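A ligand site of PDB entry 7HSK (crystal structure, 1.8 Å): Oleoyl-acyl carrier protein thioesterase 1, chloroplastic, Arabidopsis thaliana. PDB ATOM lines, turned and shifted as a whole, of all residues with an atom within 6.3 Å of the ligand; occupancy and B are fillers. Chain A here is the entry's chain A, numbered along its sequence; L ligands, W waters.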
ATOM      1  N   GLY A  41      -1.409 -19.364 -17.500  1.00  0.00           N
ATOM      2  CA  GLY A  41      -0.016 -18.929 -17.747  1.00  0.00           C
ATOM      3  C   GLY A  41       0.223 -17.489 -17.323  1.00  0.00           C
ATOM      4  O   GLY A  41       1.220 -17.207 -16.665  1.00  0.00           O
ATOM      5  N   HIS A  44      -0.240 -16.959 -13.492  1.00  0.00           N
ATOM      6  CA  HIS A  44       1.002 -17.462 -12.856  1.00  0.00           C
ATOM      7  C   HIS A  44       2.076 -16.370 -12.891  1.00  0.00           C
ATOM      8  O   HIS A  44       2.568 -16.000 -11.814  1.00  0.00           O
ATOM      9  CB  HIS A  44       1.439 -18.781 -13.512  1.00  0.00           C
ATOM     10  CG  HIS A  44       2.615 -19.386 -12.839  1.00  0.00           C
ATOM     11  ND1 HIS A  44       3.362 -20.413 -13.401  1.00  0.00           N
ATOM     12  CD2 HIS A  44       3.161 -19.123 -11.625  1.00  0.00           C
ATOM     13  CE1 HIS A  44       4.328 -20.729 -12.572  1.00  0.00           C
ATOM     14  NE2 HIS A  44       4.250 -19.936 -11.483  1.00  0.00           N
ATOM     15  N   ALA A  45       2.411 -15.825 -14.068  1.00  0.00           N
ATOM     16  CA  ALA A  45       3.324 -14.650 -14.218  1.00  0.00           C
ATOM     17  C   ALA A  45       2.967 -13.515 -13.233  1.00  0.00           C
ATOM     18  O   ALA A  45       3.877 -13.000 -12.513  1.00  0.00           O
ATOM     19  CB  ALA A  45       3.251 -14.166 -15.643  1.00  0.00           C
ATOM     20  N   GLN A  46       1.717 -13.043 -13.271  1.00  0.00           N
ATOM     21  CA  GLN A  46       1.134 -12.008 -12.367  1.00  0.00           C
ATOM     22  C   GLN A  46       1.456 -12.313 -10.892  1.00  0.00           C
ATOM     23  O   GLN A  46       1.932 -11.412 -10.136  1.00  0.00           O
ATOM     24  CB  GLN A  46      -0.388 -11.979 -12.564  1.00  0.00           C
ATOM     25  CG  GLN A  46      -1.055 -10.684 -12.116  1.00  0.00           C
ATOM     26  CD  GLN A  46      -1.144 -10.555 -10.618  1.00  0.00           C
ATOM     27  OE1 GLN A  46      -1.379 -11.522  -9.892  1.00  0.00           O
ATOM     28  NE2 GLN A  46      -0.941  -9.341 -10.148  1.00  0.00           N
ATOM     29  N   SER A  47       1.215 -13.559 -10.481  1.00  0.00           N
ATOM     30  CA  SER A  47       1.302 -14.041  -9.077  1.00  0.00           C
ATOM     31  C   SER A  47       2.727 -13.845  -8.525  1.00  0.00           C
ATOM     32  O   SER A  47       2.847 -13.811  -7.295  1.00  0.00           O
ATOM     33  CB  SER A  47       0.850 -15.470  -8.964  1.00  0.00           C
ATOM     34  OG  SER A  47       1.904 -16.356  -9.330  1.00  0.00           O
ATOM     35  N   VAL A  48       3.740 -13.756  -9.397  1.00  0.00           N
ATOM     36  CA  VAL A  48       5.173 -13.651  -8.956  1.00  0.00           C
ATOM     37  C   VAL A  48       5.905 -12.408  -9.498  1.00  0.00           C
ATOM     38  O   VAL A  48       7.152 -12.338  -9.327  1.00  0.00           O
ATOM     39  CB  VAL A  48       5.920 -14.939  -9.343  1.00  0.00           C
ATOM     40  CG1 VAL A  48       5.302 -16.160  -8.678  1.00  0.00           C
ATOM     41  CG2 VAL A  48       6.027 -15.126 -10.840  1.00  0.00           C
ATOM     42  N   PHE A  50       6.198 -10.906 -12.653  1.00  0.00           N
ATOM     43  CA  PHE A  50       6.586 -10.807 -14.089  1.00  0.00           C
ATOM     44  C   PHE A  50       5.485 -10.057 -14.864  1.00  0.00           C
ATOM     45  O   PHE A  50       4.372  -9.953 -14.295  1.00  0.00           O
ATOM     46  CB  PHE A  50       6.868 -12.181 -14.697  1.00  0.00           C
ATOM     47  CG  PHE A  50       8.054 -12.855 -14.074  1.00  0.00           C
ATOM     48  CD1 PHE A  50       9.217 -12.152 -13.826  1.00  0.00           C
ATOM     49  CD2 PHE A  50       7.987 -14.186 -13.677  1.00  0.00           C
ATOM     50  CE1 PHE A  50      10.299 -12.765 -13.207  1.00  0.00           C
ATOM     51  CE2 PHE A  50       9.076 -14.808 -13.080  1.00  0.00           C
ATOM     52  CZ  PHE A  50      10.226 -14.088 -12.824  1.00  0.00           C
ATOM     53  N   ALA A  56       5.753 -12.373 -20.240  1.00  0.00           N
ATOM     54  CA  ALA A  56       6.275 -12.798 -18.915  1.00  0.00           C
ATOM     55  C   ALA A  56       7.725 -12.346 -18.730  1.00  0.00           C
ATOM     56  O   ALA A  56       8.554 -13.181 -18.405  1.00  0.00           O
ATOM     57  CB  ALA A  56       6.161 -14.296 -18.795  1.00  0.00           C
ATOM     58  N   THR A  57       8.015 -11.047 -18.885  1.00  0.00           N
ATOM     59  CA  THR A  57       9.398 -10.475 -18.936  1.00  0.00           C
ATOM     60  C   THR A  57       9.855 -10.077 -17.529  1.00  0.00           C
ATOM     61  O   THR A  57       8.967  -9.806 -16.684  1.00  0.00           O
ATOM     62  CB  THR A  57       9.411  -9.259 -19.871  1.00  0.00           C
ATOM     63  OG1 THR A  57       8.683  -8.205 -19.260  1.00  0.00           O
ATOM     64  CG2 THR A  57       8.801  -9.574 -21.213  1.00  0.00           C
ATOM     65  N   TRP A  68       9.658 -13.348 -24.506  1.00  0.00           N
ATOM     66  CA  TRP A  68       9.463 -14.795 -24.797  1.00  0.00           C
ATOM     67  C   TRP A  68       8.411 -14.926 -25.886  1.00  0.00           C
ATOM     68  O   TRP A  68       7.370 -14.244 -25.752  1.00  0.00           O
ATOM     69  CB  TRP A  68       9.005 -15.550 -23.546  1.00  0.00           C
ATOM     70  CG  TRP A  68      10.005 -15.617 -22.444  1.00  0.00           C
ATOM     71  CD1 TRP A  68       9.977 -14.905 -21.282  1.00  0.00           C
ATOM     72  CD2 TRP A  68      11.177 -16.438 -22.394  1.00  0.00           C
ATOM     73  NE1 TRP A  68      11.050 -15.247 -20.508  1.00  0.00           N
ATOM     74  CE2 TRP A  68      11.803 -16.186 -21.159  1.00  0.00           C
ATOM     75  CE3 TRP A  68      11.753 -17.366 -23.272  1.00  0.00           C
ATOM     76  CZ2 TRP A  68      12.971 -16.823 -20.771  1.00  0.00           C
ATOM     77  CZ3 TRP A  68      12.918 -17.991 -22.889  1.00  0.00           C
ATOM     78  CH2 TRP A  68      13.521 -17.721 -21.654  1.00  0.00           C
ATOM     79  N   TRP A  92       3.292 -24.961 -14.644  1.00  0.00           N
ATOM     80  CA  TRP A  92       4.659 -24.644 -14.163  1.00  0.00           C
ATOM     81  C   TRP A  92       5.568 -24.403 -15.371  1.00  0.00           C
ATOM     82  O   TRP A  92       5.225 -24.843 -16.484  1.00  0.00           O
ATOM     83  CB  TRP A  92       5.192 -25.772 -13.263  1.00  0.00           C
ATOM     84  CG  TRP A  92       5.487 -27.065 -13.960  1.00  0.00           C
ATOM     85  CD1 TRP A  92       6.703 -27.525 -14.368  1.00  0.00           C
ATOM     86  CD2 TRP A  92       4.558 -28.122 -14.227  1.00  0.00           C
ATOM     87  NE1 TRP A  92       6.569 -28.750 -14.947  1.00  0.00           N
ATOM     88  CE2 TRP A  92       5.276 -29.156 -14.858  1.00  0.00           C
ATOM     89  CE3 TRP A  92       3.196 -28.302 -14.016  1.00  0.00           C
ATOM     90  CZ2 TRP A  92       4.676 -30.344 -15.262  1.00  0.00           C
ATOM     91  CZ3 TRP A  92       2.623 -29.504 -14.362  1.00  0.00           C
ATOM     92  CH2 TRP A  92       3.341 -30.505 -15.024  1.00  0.00           C
ATOM     93  N   CYS A  93       6.700 -23.757 -15.126  1.00  0.00           N
ATOM     94  CA  CYS A  93       7.803 -23.519 -16.083  1.00  0.00           C
ATOM     95  C   CYS A  93       9.058 -24.239 -15.623  1.00  0.00           C
ATOM     96  O   CYS A  93       9.219 -24.431 -14.403  1.00  0.00           O
ATOM     97  CB  CYS A  93       8.142 -22.040 -16.202  1.00  0.00           C
ATOM     98  SG  CYS A  93       6.889 -21.131 -17.139  1.00  0.00           S
ATOM     99  N   GLN A  94       9.960 -24.545 -16.564  1.00  0.00           N
ATOM    100  CA  GLN A  94      11.327 -25.056 -16.296  1.00  0.00           C
ATOM    101  C   GLN A  94      12.273 -24.567 -17.404  1.00  0.00           C
ATOM    102  O   GLN A  94      11.962 -24.818 -18.589  1.00  0.00           O
ATOM    103  CB  GLN A  94      11.394 -26.582 -16.309  1.00  0.00           C
ATOM    104  CG  GLN A  94      11.116 -27.231 -14.974  1.00  0.00           C
ATOM    105  CD  GLN A  94      11.768 -28.599 -14.858  1.00  0.00           C
ATOM    106  OE1 GLN A  94      11.454 -29.536 -15.600  1.00  0.00           O
ATOM    107  NE2 GLN A  94      12.667 -28.687 -13.886  1.00  0.00           N
ATOM    108  N   SER A  95      13.439 -24.037 -17.033  1.00  0.00           N
ATOM    109  CA  SER A  95      14.493 -23.668 -18.008  1.00  0.00           C
ATOM    110  C   SER A  95      15.004 -24.940 -18.685  1.00  0.00           C
ATOM    111  O   SER A  95      15.027 -25.999 -18.027  1.00  0.00           O
ATOM    112  CB  SER A  95      15.611 -22.899 -17.361  1.00  0.00           C
ATOM    113  OG  SER A  95      15.176 -21.583 -17.036  1.00  0.00           O
ATOM    114  N   GLU A  96      15.318 -24.869 -19.974  1.00  0.00           N
ATOM    115  CA  GLU A  96      16.037 -25.937 -20.709  1.00  0.00           C
ATOM    116  C   GLU A  96      17.401 -25.362 -21.085  1.00  0.00           C
ATOM    117  O   GLU A  96      17.745 -25.366 -22.259  1.00  0.00           O
ATOM    118  CB  GLU A  96      15.180 -26.473 -21.857  1.00  0.00           C
ATOM    119  CG  GLU A  96      13.953 -27.227 -21.337  1.00  0.00           C
ATOM    120  CD  GLU A  96      13.118 -27.979 -22.359  1.00  0.00           C
ATOM    121  OE1 GLU A  96      13.194 -27.625 -23.575  1.00  0.00           O
ATOM    122  OE2 GLU A  96      12.389 -28.908 -21.949  1.00  0.00           O
ATOM    123  N   GLY A 100      16.063 -22.006 -24.161  1.00  0.00           N
ATOM    124  CA  GLY A 100      14.780 -21.388 -23.790  1.00  0.00           C
ATOM    125  C   GLY A 100      14.129 -22.100 -22.605  1.00  0.00           C
ATOM    126  O   GLY A 100      14.841 -22.633 -21.753  1.00  0.00           O
ATOM    127  N   THR A 101      12.800 -22.091 -22.553  1.00  0.00           N
ATOM    128  CA  THR A 101      12.041 -22.566 -21.372  1.00  0.00           C
ATOM    129  C   THR A 101      10.853 -23.340 -21.877  1.00  0.00           C
ATOM    130  O   THR A 101      10.510 -23.205 -23.060  1.00  0.00           O
ATOM    131  CB  THR A 101      11.768 -21.388 -20.422  1.00  0.00           C
ATOM    132  OG1 THR A 101      10.555 -20.693 -20.751  1.00  0.00           O
ATOM    133  CG2 THR A 101      12.905 -20.395 -20.477  1.00  0.00           C
ATOM    134  N   ARG A 102      10.328 -24.190 -20.996  1.00  0.00           N
ATOM    135  CA  ARG A 102       9.145 -25.034 -21.229  1.00  0.00           C
ATOM    136  C   ARG A 102       8.050 -24.504 -20.310  1.00  0.00           C
ATOM    137  O   ARG A 102       8.319 -24.275 -19.082  1.00  0.00           O
ATOM    138  CB  ARG A 102       9.529 -26.486 -20.940  1.00  0.00           C
ATOM    139  CG  ARG A 102       8.817 -27.501 -21.801  1.00  0.00           C
ATOM    140  CD  ARG A 102       9.159 -28.941 -21.464  1.00  0.00           C
ATOM    141  NE  ARG A 102       8.796 -29.222 -20.070  1.00  0.00           N
ATOM    142  CZ  ARG A 102       9.635 -29.287 -19.037  1.00  0.00           C
ATOM    143  NH1 ARG A 102       9.131 -29.510 -17.838  1.00  0.00           N
ATOM    144  NH2 ARG A 102      10.930 -29.144 -19.174  1.00  0.00           N
ATOM    145  N   ARG A 103       6.845 -24.280 -20.827  1.00  0.00           N
ATOM    146  CA  ARG A 103       5.718 -24.220 -19.871  1.00  0.00           C
ATOM    147  C   ARG A 103       4.884 -25.463 -20.108  1.00  0.00           C
ATOM    148  O   ARG A 103       4.569 -25.720 -21.287  1.00  0.00           O
ATOM    149  CB  ARG A 103       4.888 -22.936 -19.974  1.00  0.00           C
ATOM    150  CG  ARG A 103       3.566 -23.052 -19.227  1.00  0.00           C
ATOM    151  CD  ARG A 103       2.819 -21.755 -19.140  1.00  0.00           C
ATOM    152  NE  ARG A 103       3.532 -20.692 -18.466  1.00  0.00           N
ATOM    153  CZ  ARG A 103       3.498 -20.446 -17.169  1.00  0.00           C
ATOM    154  NH1 ARG A 103       4.149 -19.403 -16.691  1.00  0.00           N
ATOM    155  NH2 ARG A 103       2.854 -21.239 -16.346  1.00  0.00           N
ATOM    156  N   ARG A 141      18.491 -15.971 -16.727  1.00  0.00           N
ATOM    157  CA  ARG A 141      18.214 -17.362 -16.267  1.00  0.00           C
ATOM    158  C   ARG A 141      17.921 -17.351 -14.764  1.00  0.00           C
ATOM    159  O   ARG A 141      16.839 -17.836 -14.373  1.00  0.00           O
ATOM    160  CB  ARG A 141      19.408 -18.277 -16.578  1.00  0.00           C
ATOM    161  CG  ARG A 141      19.106 -19.757 -16.462  1.00  0.00           C
ATOM    162  CD  ARG A 141      20.078 -20.610 -17.242  1.00  0.00           C
ATOM    163  NE  ARG A 141      21.434 -20.520 -16.712  1.00  0.00           N
ATOM    164  CZ  ARG A 141      22.487 -21.227 -17.156  1.00  0.00           C
ATOM    165  NH1 ARG A 141      22.339 -22.084 -18.149  1.00  0.00           N
ATOM    166  NH2 ARG A 141      23.674 -21.079 -16.587  1.00  0.00           N
ATOM    167  N   TYR A 144      14.675 -16.225 -12.972  1.00  0.00           N
ATOM    168  CA  TYR A 144      13.516 -17.168 -13.122  1.00  0.00           C
ATOM    169  C   TYR A 144      13.648 -18.460 -12.302  1.00  0.00           C
ATOM    170  O   TYR A 144      12.595 -19.074 -12.047  1.00  0.00           O
ATOM    171  CB  TYR A 144      13.346 -17.603 -14.580  1.00  0.00           C
ATOM    172  CG  TYR A 144      12.738 -16.539 -15.461  1.00  0.00           C
ATOM    173  CD1 TYR A 144      11.454 -16.089 -15.226  1.00  0.00           C
ATOM    174  CD2 TYR A 144      13.446 -15.964 -16.506  1.00  0.00           C
ATOM    175  CE1 TYR A 144      10.865 -15.114 -16.015  1.00  0.00           C
ATOM    176  CE2 TYR A 144      12.887 -14.983 -17.298  1.00  0.00           C
ATOM    177  CZ  TYR A 144      11.585 -14.557 -17.054  1.00  0.00           C
ATOM    178  OH  TYR A 144      11.008 -13.582 -17.799  1.00  0.00           O
ATOM    179  N   LEU A 145      14.860 -18.892 -11.940  1.00  0.00           N
ATOM    180  CA  LEU A 145      15.134 -20.269 -11.402  1.00  0.00           C
ATOM    181  C   LEU A 145      14.478 -20.487 -10.019  1.00  0.00           C
ATOM    182  O   LEU A 145      14.057 -21.626  -9.766  1.00  0.00           O
ATOM    183  CB  LEU A 145      16.644 -20.531 -11.337  1.00  0.00           C
ATOM    184  CG  LEU A 145      17.346 -20.744 -12.676  1.00  0.00           C
ATOM    185  CD1 LEU A 145      18.777 -21.206 -12.487  1.00  0.00           C
ATOM    186  CD2 LEU A 145      16.591 -21.717 -13.580  1.00  0.00           C
ATOM    187  N   PHE A 147      11.586 -19.562  -9.232  1.00  0.00           N
ATOM    188  CA  PHE A 147      10.122 -19.704  -9.515  1.00  0.00           C
ATOM    189  C   PHE A 147       9.807 -21.037 -10.214  1.00  0.00           C
ATOM    190  O   PHE A 147       8.612 -21.290 -10.510  1.00  0.00           O
ATOM    191  CB  PHE A 147       9.651 -18.494 -10.340  1.00  0.00           C
ATOM    192  CG  PHE A 147       9.878 -17.177  -9.632  1.00  0.00           C
ATOM    193  CD1 PHE A 147       9.198 -16.872  -8.465  1.00  0.00           C
ATOM    194  CD2 PHE A 147      10.814 -16.259 -10.098  1.00  0.00           C
ATOM    195  CE1 PHE A 147       9.404 -15.683  -7.797  1.00  0.00           C
ATOM    196  CE2 PHE A 147      11.020 -15.053  -9.428  1.00  0.00           C
ATOM    197  CZ  PHE A 147      10.309 -14.773  -8.282  1.00  0.00           C
ATOM    198  N   CYS A 148      10.824 -21.869 -10.448  1.00  0.00           N
ATOM    199  CA  CYS A 148      10.742 -23.128 -11.227  1.00  0.00           C
ATOM    200  C   CYS A 148      11.279 -24.286 -10.373  1.00  0.00           C
ATOM    201  O   CYS A 148      12.241 -24.081  -9.607  1.00  0.00           O
ATOM    202  CB  CYS A 148      11.545 -23.012 -12.527  1.00  0.00           C
ATOM    203  SG  CYS A 148      10.965 -21.685 -13.644  1.00  0.00           S
HETATM  204  N1  LIG L   1      12.457 -20.692 -16.878  1.00  0.00           N
HETATM  205  N2  LIG L   1      10.237 -19.030 -15.900  1.00  0.00           N
HETATM  206  C1  LIG L   1       8.048 -18.236 -15.064  1.00  0.00           C
HETATM  207  C2  LIG L   1       8.103 -18.913 -13.853  1.00  0.00           C
HETATM  208  C3  LIG L   1       7.085 -18.760 -12.923  1.00  0.00           C
HETATM  209  C4  LIG L   1       6.019 -17.920 -13.188  1.00  0.00           C
HETATM  210  C5  LIG L   1       5.954 -17.240 -14.371  1.00  0.00           C
HETATM  211  C6  LIG L   1      12.183 -19.365 -17.437  1.00  0.00           C
HETATM  212  C7  LIG L   1      10.843 -18.823 -17.097  1.00  0.00           C
HETATM  213  C8  LIG L   1       9.115 -18.393 -16.025  1.00  0.00           C
HETATM  214  C9  LIG L   1       6.967 -17.400 -15.296  1.00  0.00           C
HETATM  215  F1  LIG L   1       6.878 -16.717 -16.460  1.00  0.00           F
HETATM  216  N3  LIG L   1      10.174 -18.101 -17.927  1.00  0.00           N
HETATM  217  O1  LIG L   1       8.993 -17.803 -17.219  1.00  0.00           O
HETATM  218  O   HOH W   1       3.822 -16.907 -17.811  1.00  0.00           O
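A nitrogen (N1) of the ligand is in hydrogen-bond range of the side-chain hydroxyl (OG) of Ser 95, 2.9 Å away.
The backbone NH (N) of Ser 95 sits close to a nitrogen (N1) of the ligand, at 3.5 Å.
SG of Cys 148 is in hydrogen-bond range of N2 of the ligand, at 3.6 Å.
The backbone carbonyl oxygen (O) of Ala 56 lies within hydrogen-bond range of the side-chain hydroxyl (OH) of Tyr 144, at 2.6 Å.
The backbone carbonyl oxygen of His 44 sits at hydrogen-bond distance from the side-chain hydroxyl of Ser 47 (2.6 Å).
O of Tyr 144 is in hydrogen-bond range of SG of Cys 148 (3.5 Å).
The backbone carbonyl oxygen (O) of Gln 94 is in hydrogen-bond range of the backbone NH (N) of Arg 102, 3.0 Å away.
NH1 of Arg 103 is in hydrogen-bond range of SG of Cys 93 (3.3 Å).
The side-chain sulfur (SG) of Cys 148 sits close to the backbone carbonyl oxygen (O) of Cys 93 (3.3 Å).
O of Ala 45 lies within hydrogen-bond range of N of Phe 50, at 3.1 Å.
The guanidinium group (NH2) of Arg 103 sits at hydrogen-bond distance from a ring nitrogen (ND1) of His 44, at 3.1 Å.
NE2 of His 44 touches C4 of the ligand, 3.2 Å away.
Ala 45 touches the ligand.
Val 48 touches the ligand.
CD2 of Phe 50 touches C5 of the ligand (3.7 Å).
CB of Ala 56 touches F1 of the ligand (3.4 Å).
Trp 68 touches the ligand.
Cys 93 touches the ligand (CB to N2, 3.7 Å).
Gln 94 touches the ligand (C to N1, 3.9 Å).
Thr 101 touches the ligand (CG2 to C6, 3.3 Å).
Arg 103 touches the ligand (NH1 to C5, 3.6 Å).
CD1 of Tyr 144 touches N2 of the ligand (3.3 Å).
Phe 147 touches the ligand (CB to C3, 3.7 Å).
Hydrophobic or aromatic side chains within 4 Å of the ligand: His 44, Val 48, Phe 50, Ala 56, Tyr 144 and Phe 147.
The nearest printed residue that does not touch the ligand is Gly 41 (5.3 Å).
Water W1 bridges NH1 of Arg 103 (2.8 Å) and O of Gly 41 (2.9 Å).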
